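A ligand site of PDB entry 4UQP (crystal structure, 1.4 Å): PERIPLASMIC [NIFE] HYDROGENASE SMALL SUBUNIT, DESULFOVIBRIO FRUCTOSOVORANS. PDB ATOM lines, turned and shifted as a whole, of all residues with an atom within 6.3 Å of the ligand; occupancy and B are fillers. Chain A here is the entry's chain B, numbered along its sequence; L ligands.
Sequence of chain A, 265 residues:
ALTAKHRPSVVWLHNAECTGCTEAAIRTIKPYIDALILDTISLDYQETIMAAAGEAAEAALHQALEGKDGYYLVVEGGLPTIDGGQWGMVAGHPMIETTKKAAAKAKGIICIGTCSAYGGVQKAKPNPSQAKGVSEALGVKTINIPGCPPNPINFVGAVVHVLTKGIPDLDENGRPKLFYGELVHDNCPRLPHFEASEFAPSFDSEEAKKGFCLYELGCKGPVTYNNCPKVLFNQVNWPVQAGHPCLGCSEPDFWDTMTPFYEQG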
ATOM      1  N   VAL A 184       3.874 -14.843   7.233  1.00  0.00           N
ATOM      2  CA  VAL A 184       3.136 -13.824   8.009  1.00  0.00           C
ATOM      3  C   VAL A 184       2.407 -14.523   9.185  1.00  0.00           C
ATOM      4  O   VAL A 184       2.523 -14.134  10.336  1.00  0.00           O
ATOM      5  CB  VAL A 184       2.164 -13.058   7.075  1.00  0.00           C
ATOM      6  CG1 VAL A 184       1.144 -12.273   7.877  1.00  0.00           C
ATOM      7  CG2 VAL A 184       2.950 -12.141   6.153  1.00  0.00           C
ATOM      8  N   HIS A 185       1.682 -15.592   8.851  1.00  0.00           N
ATOM      9  CA  HIS A 185       0.840 -16.305   9.820  1.00  0.00           C
ATOM     10  C   HIS A 185       1.626 -16.821  11.015  1.00  0.00           C
ATOM     11  O   HIS A 185       1.108 -16.854  12.134  1.00  0.00           O
ATOM     12  CB  HIS A 185       0.186 -17.429   9.030  1.00  0.00           C
ATOM     13  CG  HIS A 185      -0.594 -18.416   9.833  1.00  0.00           C
ATOM     14  ND1 HIS A 185      -1.852 -18.151  10.325  1.00  0.00           N
ATOM     15  CD2 HIS A 185      -0.319 -19.703  10.155  1.00  0.00           C
ATOM     16  CE1 HIS A 185      -2.316 -19.229  10.936  1.00  0.00           C
ATOM     17  NE2 HIS A 185      -1.411 -20.183  10.831  1.00  0.00           N
ATOM     18  N   ASP A 186       2.835 -17.295  10.779  1.00  0.00           N
ATOM     19  CA  ASP A 186       3.585 -17.912  11.869  1.00  0.00           C
ATOM     20  C   ASP A 186       3.982 -16.959  12.986  1.00  0.00           C
ATOM     21  O   ASP A 186       4.257 -17.389  14.104  1.00  0.00           O
ATOM     22  CB  ASP A 186       4.771 -18.718  11.316  1.00  0.00           C
ATOM     23  CG  ASP A 186       4.321 -20.018  10.638  1.00  0.00           C
ATOM     24  OD1 ASP A 186       3.152 -20.461  10.797  1.00  0.00           O
ATOM     25  OD2 ASP A 186       5.160 -20.628   9.958  1.00  0.00           O
ATOM     26  N   CYS A 188       1.865 -14.178  13.564  1.00  0.00           N
ATOM     27  CA  CYS A 188       0.666 -13.369  13.785  1.00  0.00           C
ATOM     28  C   CYS A 188       0.145 -13.481  15.225  1.00  0.00           C
ATOM     29  O   CYS A 188      -0.033 -14.584  15.716  1.00  0.00           O
ATOM     30  CB  CYS A 188      -0.427 -13.802  12.805  1.00  0.00           C
ATOM     31  SG  CYS A 188      -1.953 -12.870  13.009  1.00  0.00           S
ATOM     32  N   PRO A 189      -0.126 -12.334  15.901  1.00  0.00           N
ATOM     33  CA  PRO A 189      -0.680 -12.444  17.241  1.00  0.00           C
ATOM     34  C   PRO A 189      -2.052 -13.104  17.336  1.00  0.00           C
ATOM     35  O   PRO A 189      -2.473 -13.434  18.460  1.00  0.00           O
ATOM     36  CB  PRO A 189      -0.785 -10.967  17.712  1.00  0.00           C
ATOM     37  CG  PRO A 189       0.302 -10.286  16.964  1.00  0.00           C
ATOM     38  CD  PRO A 189       0.209 -10.938  15.584  1.00  0.00           C
ATOM     39  N   ARG A 190      -2.744 -13.293  16.205  1.00  0.00           N
ATOM     40  CA  ARG A 190      -4.038 -13.998  16.221  1.00  0.00           C
ATOM     41  C   ARG A 190      -3.875 -15.501  16.075  1.00  0.00           C
ATOM     42  O   ARG A 190      -4.871 -16.232  16.049  1.00  0.00           O
ATOM     43  CB  ARG A 190      -4.970 -13.448  15.160  1.00  0.00           C
ATOM     44  CG  ARG A 190      -5.254 -11.961  15.396  1.00  0.00           C
ATOM     45  CD  ARG A 190      -6.422 -11.398  14.610  1.00  0.00           C
ATOM     46  NE  ARG A 190      -6.508  -9.950  14.845  1.00  0.00           N
ATOM     47  CZ  ARG A 190      -7.598  -9.211  14.638  1.00  0.00           C
ATOM     48  NH1 ARG A 190      -8.701  -9.748  14.162  1.00  0.00           N
ATOM     49  NH2 ARG A 190      -7.592  -7.894  14.901  1.00  0.00           N
ATOM     50  N   LEU A 191      -2.632 -15.974  15.974  1.00  0.00           N
ATOM     51  CA  LEU A 191      -2.353 -17.417  15.784  1.00  0.00           C
ATOM     52  C   LEU A 191      -3.012 -18.306  16.857  1.00  0.00           C
ATOM     53  O   LEU A 191      -3.574 -19.332  16.492  1.00  0.00           O
ATOM     54  CB  LEU A 191      -0.849 -17.686  15.649  1.00  0.00           C
ATOM     55  CG  LEU A 191      -0.458 -19.138  15.338  1.00  0.00           C
ATOM     56  CD1 LEU A 191      -1.039 -19.548  14.011  1.00  0.00           C
ATOM     57  CD2 LEU A 191       1.072 -19.244  15.327  1.00  0.00           C
ATOM     58  N   PRO A 192      -3.017 -17.906  18.142  1.00  0.00           N
ATOM     59  CA  PRO A 192      -3.727 -18.756  19.118  1.00  0.00           C
ATOM     60  C   PRO A 192      -5.222 -18.904  18.796  1.00  0.00           C
ATOM     61  O   PRO A 192      -5.809 -19.961  19.052  1.00  0.00           O
ATOM     62  CB  PRO A 192      -3.494 -18.037  20.453  1.00  0.00           C
ATOM     63  CG  PRO A 192      -2.219 -17.290  20.235  1.00  0.00           C
ATOM     64  CD  PRO A 192      -2.279 -16.811  18.811  1.00  0.00           C
ATOM     65  N   HIS A 193      -5.835 -17.880  18.221  1.00  0.00           N
ATOM     66  CA  HIS A 193      -7.237 -18.001  17.781  1.00  0.00           C
ATOM     67  C   HIS A 193      -7.346 -18.977  16.623  1.00  0.00           C
ATOM     68  O   HIS A 193      -8.236 -19.828  16.598  1.00  0.00           O
ATOM     69  CB  HIS A 193      -7.873 -16.652  17.410  1.00  0.00           C
ATOM     70  CG  HIS A 193      -8.141 -15.755  18.573  1.00  0.00           C
ATOM     71  ND1 HIS A 193      -8.879 -16.146  19.683  1.00  0.00           N
ATOM     72  CD2 HIS A 193      -7.795 -14.465  18.796  1.00  0.00           C
ATOM     73  CE1 HIS A 193      -8.963 -15.135  20.522  1.00  0.00           C
ATOM     74  NE2 HIS A 193      -8.313 -14.106  20.017  1.00  0.00           N
ATOM     75  N   PHE A 194      -6.459 -18.833  15.635  1.00  0.00           N
ATOM     76  CA  PHE A 194      -6.486 -19.757  14.502  1.00  0.00           C
ATOM     77  C   PHE A 194      -6.393 -21.208  14.990  1.00  0.00           C
ATOM     78  O   PHE A 194      -7.187 -22.047  14.605  1.00  0.00           O
ATOM     79  CB  PHE A 194      -5.339 -19.443  13.534  1.00  0.00           C
ATOM     80  CG  PHE A 194      -5.186 -20.430  12.414  1.00  0.00           C
ATOM     81  CD1 PHE A 194      -5.900 -20.255  11.227  1.00  0.00           C
ATOM     82  CD2 PHE A 194      -4.299 -21.504  12.521  1.00  0.00           C
ATOM     83  CE1 PHE A 194      -5.758 -21.152  10.168  1.00  0.00           C
ATOM     84  CE2 PHE A 194      -4.126 -22.404  11.455  1.00  0.00           C
ATOM     85  CZ  PHE A 194      -4.848 -22.220  10.276  1.00  0.00           C
ATOM     86  N   PHE A 199     -12.715 -17.855  14.765  1.00  0.00           N
ATOM     87  CA  PHE A 199     -12.722 -17.047  13.546  1.00  0.00           C
ATOM     88  C   PHE A 199     -13.829 -16.001  13.569  1.00  0.00           C
ATOM     89  O   PHE A 199     -14.932 -16.262  14.038  1.00  0.00           O
ATOM     90  CB  PHE A 199     -12.957 -17.929  12.321  1.00  0.00           C
ATOM     91  CG  PHE A 199     -11.961 -19.046  12.151  1.00  0.00           C
ATOM     92  CD1 PHE A 199     -10.637 -18.761  11.835  1.00  0.00           C
ATOM     93  CD2 PHE A 199     -12.344 -20.362  12.294  1.00  0.00           C
ATOM     94  CE1 PHE A 199      -9.716 -19.792  11.669  1.00  0.00           C
ATOM     95  CE2 PHE A 199     -11.433 -21.392  12.157  1.00  0.00           C
ATOM     96  CZ  PHE A 199     -10.109 -21.106  11.840  1.00  0.00           C
ATOM     97  N   PHE A 212     -10.685 -12.029  16.781  1.00  0.00           N
ATOM     98  CA  PHE A 212     -10.545 -13.438  16.336  1.00  0.00           C
ATOM     99  C   PHE A 212      -9.835 -13.486  14.973  1.00  0.00           C
ATOM    100  O   PHE A 212      -9.690 -12.470  14.257  1.00  0.00           O
ATOM    101  CB  PHE A 212     -11.913 -14.109  16.239  1.00  0.00           C
ATOM    102  CG  PHE A 212     -12.469 -14.622  17.556  1.00  0.00           C
ATOM    103  CD1 PHE A 212     -12.013 -14.170  18.792  1.00  0.00           C
ATOM    104  CD2 PHE A 212     -13.505 -15.557  17.524  1.00  0.00           C
ATOM    105  CE1 PHE A 212     -12.568 -14.645  19.983  1.00  0.00           C
ATOM    106  CE2 PHE A 212     -14.058 -16.055  18.707  1.00  0.00           C
ATOM    107  CZ  PHE A 212     -13.594 -15.582  19.937  1.00  0.00           C
ATOM    108  N   CYS A 213      -9.355 -14.681  14.609  1.00  0.00           N
ATOM    109  CA  CYS A 213      -8.594 -14.860  13.380  1.00  0.00           C
ATOM    110  C   CYS A 213      -9.441 -14.517  12.159  1.00  0.00           C
ATOM    111  O   CYS A 213     -10.665 -14.719  12.149  1.00  0.00           O
ATOM    112  CB  CYS A 213      -8.107 -16.318  13.340  1.00  0.00           C
ATOM    113  SG  CYS A 213      -7.421 -16.824  11.751  1.00  0.00           S
ATOM    114  N   LEU A 214      -8.798 -13.978  11.129  1.00  0.00           N
ATOM    115  CA  LEU A 214      -9.457 -13.460   9.921  1.00  0.00           C
ATOM    116  C   LEU A 214      -9.452 -14.444   8.735  1.00  0.00           C
ATOM    117  O   LEU A 214      -9.736 -14.069   7.586  1.00  0.00           O
ATOM    118  CB  LEU A 214      -8.746 -12.168   9.524  1.00  0.00           C
ATOM    119  CG  LEU A 214      -8.811 -11.082  10.616  1.00  0.00           C
ATOM    120  CD1 LEU A 214      -8.055  -9.840  10.181  1.00  0.00           C
ATOM    121  CD2 LEU A 214     -10.254 -10.706  10.978  1.00  0.00           C
ATOM    122  N   TYR A 215      -9.089 -15.691   8.996  1.00  0.00           N
ATOM    123  CA  TYR A 215      -8.963 -16.694   7.924  1.00  0.00           C
ATOM    124  C   TYR A 215     -10.243 -16.877   7.100  1.00  0.00           C
ATOM    125  O   TYR A 215     -10.192 -17.027   5.873  1.00  0.00           O
ATOM    126  CB  TYR A 215      -8.450 -18.034   8.472  1.00  0.00           C
ATOM    127  CG  TYR A 215      -7.972 -18.971   7.386  1.00  0.00           C
ATOM    128  CD1 TYR A 215      -6.736 -18.808   6.771  1.00  0.00           C
ATOM    129  CD2 TYR A 215      -8.795 -20.013   6.925  1.00  0.00           C
ATOM    130  CE1 TYR A 215      -6.298 -19.677   5.760  1.00  0.00           C
ATOM    131  CE2 TYR A 215      -8.385 -20.871   5.914  1.00  0.00           C
ATOM    132  CZ  TYR A 215      -7.138 -20.707   5.335  1.00  0.00           C
ATOM    133  OH  TYR A 215      -6.720 -21.546   4.318  1.00  0.00           O
ATOM    134  N   CYS A 219      -7.971 -14.237   4.802  1.00  0.00           N
ATOM    135  CA  CYS A 219      -6.576 -13.921   5.148  1.00  0.00           C
ATOM    136  C   CYS A 219      -5.610 -14.867   4.456  1.00  0.00           C
ATOM    137  O   CYS A 219      -5.710 -16.099   4.565  1.00  0.00           O
ATOM    138  CB  CYS A 219      -6.375 -13.997   6.647  1.00  0.00           C
ATOM    139  SG  CYS A 219      -4.763 -13.338   7.135  1.00  0.00           S
ATOM    140  N   LYS A 220      -4.655 -14.262   3.744  1.00  0.00           N
ATOM    141  CA  LYS A 220      -3.622 -15.044   3.056  1.00  0.00           C
ATOM    142  C   LYS A 220      -2.319 -15.129   3.858  1.00  0.00           C
ATOM    143  O   LYS A 220      -1.320 -15.619   3.364  1.00  0.00           O
ATOM    144  CB  LYS A 220      -3.374 -14.471   1.662  1.00  0.00           C
ATOM    145  CG  LYS A 220      -4.635 -14.388   0.797  1.00  0.00           C
ATOM    146  CD  LYS A 220      -5.336 -15.758   0.693  1.00  0.00           C
ATOM    147  CE  LYS A 220      -6.468 -15.784  -0.333  1.00  0.00           C
ATOM    148  NZ  LYS A 220      -7.462 -14.690  -0.171  1.00  0.00           N
ATOM    149  N   GLY A 221      -2.341 -14.715   5.122  1.00  0.00           N
ATOM    150  CA  GLY A 221      -1.176 -14.861   5.975  1.00  0.00           C
ATOM    151  C   GLY A 221      -0.550 -16.255   5.947  1.00  0.00           C
ATOM    152  O   GLY A 221       0.664 -16.386   5.945  1.00  0.00           O
ATOM    153  N   PRO A 222      -1.385 -17.315   5.960  1.00  0.00           N
ATOM    154  CA  PRO A 222      -0.847 -18.688   5.954  1.00  0.00           C
ATOM    155  C   PRO A 222      -0.068 -19.120   4.703  1.00  0.00           C
ATOM    156  O   PRO A 222       0.582 -20.174   4.731  1.00  0.00           O
ATOM    157  CB  PRO A 222      -2.078 -19.555   6.165  1.00  0.00           C
ATOM    158  CG  PRO A 222      -3.016 -18.654   6.939  1.00  0.00           C
ATOM    159  CD  PRO A 222      -2.833 -17.318   6.278  1.00  0.00           C
ATOM    160  N   TRP A 238      -0.059  -3.100  11.562  1.00  0.00           N
ATOM    161  CA  TRP A 238      -0.033  -3.900  10.324  1.00  0.00           C
ATOM    162  C   TRP A 238      -1.468  -4.302  10.009  1.00  0.00           C
ATOM    163  O   TRP A 238      -2.350  -4.154  10.859  1.00  0.00           O
ATOM    164  CB  TRP A 238       0.959  -5.069  10.399  1.00  0.00           C
ATOM    165  CG  TRP A 238       0.525  -6.219  11.274  1.00  0.00           C
ATOM    166  CD1 TRP A 238       0.421  -6.225  12.647  1.00  0.00           C
ATOM    167  CD2 TRP A 238       0.210  -7.537  10.837  1.00  0.00           C
ATOM    168  NE1 TRP A 238       0.042  -7.478  13.071  1.00  0.00           N
ATOM    169  CE2 TRP A 238      -0.106  -8.295  11.979  1.00  0.00           C
ATOM    170  CE3 TRP A 238       0.133  -8.142   9.575  1.00  0.00           C
ATOM    171  CZ2 TRP A 238      -0.474  -9.654  11.900  1.00  0.00           C
ATOM    172  CZ3 TRP A 238      -0.212  -9.495   9.497  1.00  0.00           C
ATOM    173  CH2 TRP A 238      -0.520 -10.234  10.660  1.00  0.00           C
ATOM    174  N   VAL A 240      -3.485  -6.953   9.793  1.00  0.00           N
ATOM    175  CA  VAL A 240      -4.321  -7.799  10.683  1.00  0.00           C
ATOM    176  C   VAL A 240      -4.576  -7.113  12.032  1.00  0.00           C
ATOM    177  O   VAL A 240      -5.675  -7.246  12.608  1.00  0.00           O
ATOM    178  CB  VAL A 240      -3.694  -9.197  10.832  1.00  0.00           C
ATOM    179  CG1 VAL A 240      -4.316  -9.984  11.982  1.00  0.00           C
ATOM    180  CG2 VAL A 240      -3.826  -9.960   9.516  1.00  0.00           C
ATOM    181  N   PRO A 245      -7.815  -8.829   6.674  1.00  0.00           N
ATOM    182  CA  PRO A 245      -6.976  -9.933   6.220  1.00  0.00           C
ATOM    183  C   PRO A 245      -5.781  -9.487   5.380  1.00  0.00           C
ATOM    184  O   PRO A 245      -5.808  -8.451   4.713  1.00  0.00           O
ATOM    185  CB  PRO A 245      -7.939 -10.787   5.351  1.00  0.00           C
ATOM    186  CG  PRO A 245      -9.068  -9.853   5.006  1.00  0.00           C
ATOM    187  CD  PRO A 245      -9.214  -8.972   6.212  1.00  0.00           C
ATOM    188  N   CYS A 246      -4.720 -10.273   5.436  1.00  0.00           N
ATOM    189  CA  CYS A 246      -3.603 -10.169   4.519  1.00  0.00           C
ATOM    190  C   CYS A 246      -4.062 -10.534   3.104  1.00  0.00           C
ATOM    191  O   CYS A 246      -4.839 -11.481   2.911  1.00  0.00           O
ATOM    192  CB  CYS A 246      -2.508 -11.145   5.003  1.00  0.00           C
ATOM    193  SG  CYS A 246      -1.032 -11.285   3.954  1.00  0.00           S
ATOM    194  N   GLN A 264     -11.277 -17.971   0.505  1.00  0.00           N
ATOM    195  CA  GLN A 264     -10.148 -18.890   0.384  1.00  0.00           C
ATOM    196  C   GLN A 264     -10.310 -19.649  -0.953  1.00  0.00           C
ATOM    197  O   GLN A 264     -10.793 -20.762  -0.975  1.00  0.00           O
ATOM    198  CB  GLN A 264     -10.093 -19.835   1.610  1.00  0.00           C
ATOM    199  CG  GLN A 264      -9.761 -19.135   2.930  1.00  0.00           C
ATOM    200  CD  GLN A 264      -8.383 -18.462   2.943  1.00  0.00           C
ATOM    201  OE1 GLN A 264      -7.496 -18.780   2.139  1.00  0.00           O
ATOM    202  NE2 GLN A 264      -8.196 -17.528   3.872  1.00  0.00           N
HETATM  203 FE1  LIG L   1      -5.469 -15.736  11.312  1.00  0.00          FE
HETATM  204 FE2  LIG L   1      -3.308 -14.105  11.666  1.00  0.00          FE
HETATM  205 FE3  LIG L   1      -3.047 -16.414  10.333  1.00  0.00          FE
HETATM  206 FE4  LIG L   1      -4.389 -14.333   9.162  1.00  0.00          FE
HETATM  207  S1  LIG L   1      -2.173 -14.433   9.661  1.00  0.00           S
HETATM  208  S2  LIG L   1      -5.000 -16.544   9.185  1.00  0.00           S
HETATM  209  S3  LIG L   1      -5.417 -13.451  11.075  1.00  0.00           S
HETATM  210  S4  LIG L   1      -3.635 -16.193  12.557  1.00  0.00           S
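A ring nitrogen (ND1) of His 185 is bound to an iron atom (FE3) of the ligand (2.1 Å).
An iron atom (FE2) of the ligand is bound by the side-chain sulfur (SG) of Cys 188 (2.3 Å).
The side-chain sulfur of Cys 213 binds an iron atom (FE1) of the ligand, at 2.3 Å.
SG of Cys 219 binds FE4 of the ligand, at 2.3 Å.
The backbone NH of Leu 214 lies close to a sulfur (S3) of the ligand (3.4 Å).
S4 of the ligand sits close to N of Leu 191 (3.6 Å).
The backbone carbonyl oxygen of Gly 221 lies within hydrogen-bond range of the backbone NH of His 185 (3.2 Å).
N of Arg 190 lies close to SG of Cys 188 (3.3 Å).
The side-chain sulfur (SG) of Cys 213 sits close to the backbone NH (N) of Tyr 215 (3.4 Å).
The side-chain sulfur (SG) of Cys 219 lies close to the backbone NH (N) of Cys 246 (3.5 Å).
The side-chain amide nitrogen of Gln 264 is in hydrogen-bond range of the backbone carbonyl oxygen of Cys 219, 2.9 Å away.
The guanidinium group (NH2) of Arg 190 is in hydrogen-bond range of the backbone carbonyl oxygen (O) of Val 240 (3.1 Å).
The backbone carbonyl oxygen (O) of Phe 212 sits at hydrogen-bond distance from the guanidinium group (NH1) of Arg 190, at 2.9 Å.
The backbone carbonyl oxygen of Tyr 215 lies within hydrogen-bond range of the side-chain amide nitrogen of Gln 264, 2.9 Å away.
The backbone carbonyl oxygen (O) of Arg 190 sits close to a sulfur (S4) of the ligand (3.7 Å).
CB of Phe 194 touches S4 of the ligand, at 3.8 Å.
Tyr 215 touches the ligand.
Gly 221 touches the ligand (CA to S1, 3.8 Å).
CG of Pro 222 touches S2 of the ligand, at 3.7 Å.
CG1 of Val 240 touches S3 of the ligand (3.7 Å).
Hydrophobic or aromatic side chains that line the ligand: His 185, Phe 194, Leu 214, Tyr 215, Pro 222 and Val 240.
Within 4 Å of the ligand: His 185, Cys 188, Arg 190, Leu 191, Phe 194, Cys 213, Leu 214, Tyr 215, Cys 219, Gly 221, Pro 222 and Val 240.
The nearest printed residue that does not touch the ligand is Val 184 (4.3 Å).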
